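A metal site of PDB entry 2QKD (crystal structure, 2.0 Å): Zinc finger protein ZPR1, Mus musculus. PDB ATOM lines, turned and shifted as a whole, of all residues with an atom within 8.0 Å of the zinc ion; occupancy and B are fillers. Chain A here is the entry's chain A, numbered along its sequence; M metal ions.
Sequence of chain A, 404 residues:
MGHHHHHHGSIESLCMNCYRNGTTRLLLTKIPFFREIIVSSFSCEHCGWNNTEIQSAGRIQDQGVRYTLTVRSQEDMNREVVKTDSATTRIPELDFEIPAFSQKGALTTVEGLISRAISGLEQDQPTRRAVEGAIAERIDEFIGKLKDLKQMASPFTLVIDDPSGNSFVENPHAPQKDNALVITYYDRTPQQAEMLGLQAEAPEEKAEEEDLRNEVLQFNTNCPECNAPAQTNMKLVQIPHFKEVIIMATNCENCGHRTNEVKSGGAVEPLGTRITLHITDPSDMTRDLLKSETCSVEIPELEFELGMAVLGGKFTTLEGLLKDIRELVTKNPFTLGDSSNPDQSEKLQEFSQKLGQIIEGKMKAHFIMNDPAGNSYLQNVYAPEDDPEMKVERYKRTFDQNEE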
ATOM      1  N   ASN A 222      10.701  -3.649  19.787  1.00  0.00           N
ATOM      2  CA  ASN A 222       9.547  -4.422  19.294  1.00  0.00           C
ATOM      3  C   ASN A 222       9.076  -4.057  17.884  1.00  0.00           C
ATOM      4  O   ASN A 222       9.297  -2.939  17.396  1.00  0.00           O
ATOM      5  CB  ASN A 222       8.374  -4.320  20.273  1.00  0.00           C
ATOM      6  CG  ASN A 222       8.683  -4.933  21.621  1.00  0.00           C
ATOM      7  OD1 ASN A 222       8.379  -6.105  21.877  1.00  0.00           O
ATOM      8  ND2 ASN A 222       9.293  -4.144  22.509  1.00  0.00           N
ATOM      9  N   CYS A 223       8.427  -5.030  17.229  1.00  0.00           N
ATOM     10  CA  CYS A 223       7.681  -4.775  15.995  1.00  0.00           C
ATOM     11  C   CYS A 223       6.460  -3.888  16.323  1.00  0.00           C
ATOM     12  O   CYS A 223       5.599  -4.287  17.120  1.00  0.00           O
ATOM     13  CB  CYS A 223       7.295  -6.101  15.332  1.00  0.00           C
ATOM     14  SG  CYS A 223       5.671  -6.271  14.505  1.00  0.00           S
ATOM     15  N   PRO A 224       6.412  -2.678  15.729  1.00  0.00           N
ATOM     16  CA  PRO A 224       5.387  -1.661  16.037  1.00  0.00           C
ATOM     17  C   PRO A 224       3.953  -2.038  15.642  1.00  0.00           C
ATOM     18  O   PRO A 224       3.033  -1.255  15.862  1.00  0.00           O
ATOM     19  CB  PRO A 224       5.849  -0.457  15.221  1.00  0.00           C
ATOM     20  CG  PRO A 224       6.637  -1.036  14.092  1.00  0.00           C
ATOM     21  CD  PRO A 224       7.346  -2.200  14.693  1.00  0.00           C
ATOM     22  N   GLU A 225       3.766  -3.233  15.078  1.00  0.00           N
ATOM     23  CA  GLU A 225       2.431  -3.711  14.705  1.00  0.00           C
ATOM     24  C   GLU A 225       2.096  -4.997  15.457  1.00  0.00           C
ATOM     25  O   GLU A 225       0.995  -5.141  15.990  1.00  0.00           O
ATOM     26  CB  GLU A 225       2.351  -3.938  13.196  1.00  0.00           C
ATOM     27  CG  GLU A 225       0.921  -4.012  12.649  1.00  0.00           C
ATOM     28  CD  GLU A 225       0.849  -4.522  11.216  1.00  0.00           C
ATOM     29  OE1 GLU A 225       1.740  -5.287  10.799  1.00  0.00           O
ATOM     30  OE2 GLU A 225      -0.117  -4.156  10.508  1.00  0.00           O
ATOM     31  N   CYS A 226       3.050  -5.914  15.494  1.00  0.00           N
ATOM     32  CA  CYS A 226       2.818  -7.252  16.029  1.00  0.00           C
ATOM     33  C   CYS A 226       3.417  -7.467  17.407  1.00  0.00           C
ATOM     34  O   CYS A 226       3.203  -8.520  18.023  1.00  0.00           O
ATOM     35  CB  CYS A 226       3.381  -8.280  15.049  1.00  0.00           C
ATOM     36  SG  CYS A 226       5.183  -8.223  14.924  1.00  0.00           S
ATOM     37  N   ASN A 227       4.181  -6.489  17.886  1.00  0.00           N
ATOM     38  CA  ASN A 227       4.851  -6.567  19.195  1.00  0.00           C
ATOM     39  C   ASN A 227       5.876  -7.708  19.318  1.00  0.00           C
ATOM     40  O   ASN A 227       6.288  -8.059  20.426  1.00  0.00           O
ATOM     41  CB  ASN A 227       3.815  -6.636  20.330  1.00  0.00           C
ATOM     42  CG  ASN A 227       4.365  -6.162  21.678  1.00  0.00           C
ATOM     43  OD1 ASN A 227       5.530  -5.785  21.791  1.00  0.00           O
ATOM     44  ND2 ASN A 227       3.525  -6.195  22.696  1.00  0.00           N
ATOM     45  N   ALA A 228       6.269  -8.275  18.180  1.00  0.00           N
ATOM     46  CA  ALA A 228       7.325  -9.297  18.168  1.00  0.00           C
ATOM     47  C   ALA A 228       8.603  -8.707  18.777  1.00  0.00           C
ATOM     48  O   ALA A 228       8.802  -7.491  18.734  1.00  0.00           O
ATOM     49  CB  ALA A 228       7.594  -9.788  16.756  1.00  0.00           C
ATOM     50  N   PRO A 229       9.477  -9.564  19.353  1.00  0.00           N
ATOM     51  CA  PRO A 229      10.616  -8.966  20.043  1.00  0.00           C
ATOM     52  C   PRO A 229      11.801  -8.724  19.117  1.00  0.00           C
ATOM     53  O   PRO A 229      12.102  -9.548  18.255  1.00  0.00           O
ATOM     54  CB  PRO A 229      10.949  -9.993  21.125  1.00  0.00           C
ATOM     55  CG  PRO A 229      10.316 -11.308  20.652  1.00  0.00           C
ATOM     56  CD  PRO A 229       9.507 -11.037  19.414  1.00  0.00           C
ATOM     57  N   GLN A 231      12.530  -6.873  16.555  1.00  0.00           N
ATOM     58  CA  GLN A 231      12.375  -6.842  15.089  1.00  0.00           C
ATOM     59  C   GLN A 231      12.633  -5.484  14.444  1.00  0.00           C
ATOM     60  O   GLN A 231      12.829  -5.403  13.224  1.00  0.00           O
ATOM     61  CB  GLN A 231      10.987  -7.374  14.665  1.00  0.00           C
ATOM     62  CG  GLN A 231      10.763  -8.893  14.846  1.00  0.00           C
ATOM     63  CD  GLN A 231      11.960  -9.730  14.443  1.00  0.00           C
ATOM     64  OE1 GLN A 231      12.370  -9.751  13.280  1.00  0.00           O
ATOM     65  NE2 GLN A 231      12.541 -10.429  15.408  1.00  0.00           N
ATOM     66  N   THR A 232      12.627  -4.412  15.242  1.00  0.00           N
ATOM     67  CA  THR A 232      12.891  -3.052  14.740  1.00  0.00           C
ATOM     68  C   THR A 232      14.213  -2.524  15.284  1.00  0.00           C
ATOM     69  O   THR A 232      14.441  -2.535  16.489  1.00  0.00           O
ATOM     70  CB  THR A 232      11.766  -2.080  15.151  1.00  0.00           C
ATOM     71  OG1 THR A 232      10.524  -2.499  14.569  1.00  0.00           O
ATOM     72  CG2 THR A 232      12.075  -0.644  14.706  1.00  0.00           C
ATOM     73  N   THR A 250      12.526  -1.429  10.380  1.00  0.00           N
ATOM     74  CA  THR A 250      11.912  -2.711  10.700  1.00  0.00           C
ATOM     75  C   THR A 250      12.104  -3.728   9.577  1.00  0.00           C
ATOM     76  O   THR A 250      12.256  -3.359   8.414  1.00  0.00           O
ATOM     77  CB  THR A 250      10.419  -2.543  11.032  1.00  0.00           C
ATOM     78  OG1 THR A 250      10.273  -1.550  12.057  1.00  0.00           O
ATOM     79  CG2 THR A 250       9.811  -3.850  11.531  1.00  0.00           C
ATOM     80  N   ASN A 251      12.152  -5.001   9.960  1.00  0.00           N
ATOM     81  CA  ASN A 251      12.184  -6.132   9.030  1.00  0.00           C
ATOM     82  C   ASN A 251      11.767  -7.370   9.822  1.00  0.00           C
ATOM     83  O   ASN A 251      12.596  -8.089  10.390  1.00  0.00           O
ATOM     84  CB  ASN A 251      13.567  -6.291   8.388  1.00  0.00           C
ATOM     85  CG  ASN A 251      13.477  -6.729   6.930  1.00  0.00           C
ATOM     86  OD1 ASN A 251      12.936  -7.791   6.617  1.00  0.00           O
ATOM     87  ND2 ASN A 251      14.016  -5.911   6.031  1.00  0.00           N
ATOM     88  N   CYS A 252      10.459  -7.592   9.867  1.00  0.00           N
ATOM     89  CA  CYS A 252       9.823  -8.550  10.755  1.00  0.00           C
ATOM     90  C   CYS A 252      10.029  -9.996  10.282  1.00  0.00           C
ATOM     91  O   CYS A 252       9.834 -10.303   9.116  1.00  0.00           O
ATOM     92  CB  CYS A 252       8.341  -8.221  10.845  1.00  0.00           C
ATOM     93  SG  CYS A 252       7.369  -9.087  12.068  1.00  0.00           S
ATOM     94  N   GLU A 253      10.429 -10.872  11.214  1.00  0.00           N
ATOM     95  CA  GLU A 253      10.627 -12.294  10.919  1.00  0.00           C
ATOM     96  C   GLU A 253       9.379 -13.116  11.242  1.00  0.00           C
ATOM     97  O   GLU A 253       9.182 -14.209  10.705  1.00  0.00           O
ATOM     98  CB  GLU A 253      11.817 -12.860  11.697  1.00  0.00           C
ATOM     99  CG  GLU A 253      13.177 -12.536  11.095  1.00  0.00           C
ATOM    100  CD  GLU A 253      14.329 -13.143  11.886  1.00  0.00           C
ATOM    101  OE1 GLU A 253      15.495 -12.876  11.519  1.00  0.00           O
ATOM    102  OE2 GLU A 253      14.074 -13.877  12.867  1.00  0.00           O
ATOM    103  N   ASN A 254       8.540 -12.587  12.134  1.00  0.00           N
ATOM    104  CA  ASN A 254       7.343 -13.276  12.584  1.00  0.00           C
ATOM    105  C   ASN A 254       6.077 -12.820  11.868  1.00  0.00           C
ATOM    106  O   ASN A 254       5.030 -13.460  11.973  1.00  0.00           O
ATOM    107  CB  ASN A 254       7.183 -13.116  14.099  1.00  0.00           C
ATOM    108  CG  ASN A 254       8.343 -13.699  14.885  1.00  0.00           C
ATOM    109  OD1 ASN A 254       9.214 -12.966  15.374  1.00  0.00           O
ATOM    110  ND2 ASN A 254       8.372 -15.030  15.006  1.00  0.00           N
ATOM    111  N   CYS A 255       6.177 -11.717  11.128  1.00  0.00           N
ATOM    112  CA  CYS A 255       5.001 -11.075  10.548  1.00  0.00           C
ATOM    113  C   CYS A 255       5.249 -10.454   9.170  1.00  0.00           C
ATOM    114  O   CYS A 255       4.308 -10.048   8.483  1.00  0.00           O
ATOM    115  CB  CYS A 255       4.458 -10.020  11.504  1.00  0.00           C
ATOM    116  SG  CYS A 255       5.460  -8.490  11.594  1.00  0.00           S
ATOM    117  N   GLY A 256       6.524 -10.373   8.781  1.00  0.00           N
ATOM    118  CA  GLY A 256       6.918  -9.849   7.464  1.00  0.00           C
ATOM    119  C   GLY A 256       6.839  -8.339   7.271  1.00  0.00           C
ATOM    120  O   GLY A 256       7.246  -7.825   6.220  1.00  0.00           O
ATOM    121  N   HIS A 257       6.311  -7.633   8.273  1.00  0.00           N
ATOM    122  CA  HIS A 257       6.139  -6.168   8.231  1.00  0.00           C
ATOM    123  C   HIS A 257       7.475  -5.430   8.122  1.00  0.00           C
ATOM    124  O   HIS A 257       8.347  -5.567   8.975  1.00  0.00           O
ATOM    125  CB  HIS A 257       5.329  -5.703   9.452  1.00  0.00           C
ATOM    126  CG  HIS A 257       5.107  -4.218   9.520  1.00  0.00           C
ATOM    127  ND1 HIS A 257       5.030  -3.419   8.404  1.00  0.00           N
ATOM    128  CD2 HIS A 257       4.905  -3.405  10.579  1.00  0.00           C
ATOM    129  CE1 HIS A 257       4.810  -2.168   8.768  1.00  0.00           C
ATOM    130  NE2 HIS A 257       4.732  -2.132  10.089  1.00  0.00           N
ATOM    131  N   ARG A 258       7.611  -4.646   7.046  1.00  0.00           N
ATOM    132  CA  ARG A 258       8.856  -3.967   6.693  1.00  0.00           C
ATOM    133  C   ARG A 258       8.647  -2.468   6.496  1.00  0.00           C
ATOM    134  O   ARG A 258       7.813  -2.053   5.680  1.00  0.00           O
ATOM    135  CB  ARG A 258       9.432  -4.604   5.410  1.00  0.00           C
ATOM    136  CG  ARG A 258      10.611  -3.889   4.761  1.00  0.00           C
ATOM    137  CD  ARG A 258      10.975  -4.537   3.420  1.00  0.00           C
ATOM    138  NE  ARG A 258      12.233  -4.046   2.851  1.00  0.00           N
ATOM    139  CZ  ARG A 258      12.828  -4.567   1.773  1.00  0.00           C
ATOM    140  NH1 ARG A 258      12.276  -5.587   1.121  1.00  0.00           N
ATOM    141  NH2 ARG A 258      13.967  -4.071   1.336  1.00  0.00           N
HETATM  142 ZN    ZN M   1       6.339  -7.777  13.103  1.00  0.00          ZN
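SG of Cys 255 is bound to the zinc ion. SG of Cys 252 binds the zinc ion, at 2.0 Å. The zinc ion is bound by SG of Cys 223 (2.2 Å). The side-chain sulfur (SG) of Cys 226 is bound to the zinc ion (2.2 Å). The zinc ion has four donor atoms within binding distance.
Within 4 Å of the zinc ion: Cys 223, Cys 226, Cys 252 and Cys 255. The nearest printed residue that does not touch the zinc ion is His 257 (4.3 Å).
The side-chain sulfur of Cys 252 is disulfide-bonded to the side-chain sulfur of Cys 255 (2.1 Å). The side-chain sulfur (SG) of Cys 255 sits close to the backbone NH (N) of His 257 (3.5 Å). The backbone NH (N) of Gly 256 lies close to the side-chain sulfur (SG) of Cys 252 (3.6 Å). The side-chain sulfur of Cys 252 sits close to the backbone NH of Asn 254 (3.7 Å). O of Ala 228 sits at hydrogen-bond distance from N of Cys 223, 2.9 Å away. SG of Cys 223 lies close to N of Asn 227, 3.7 Å away. N of Glu 225 lies close to SG of Cys 223, at 3.6 Å. The backbone NH (N) of Ala 228 sits close to the side-chain sulfur (SG) of Cys 226.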
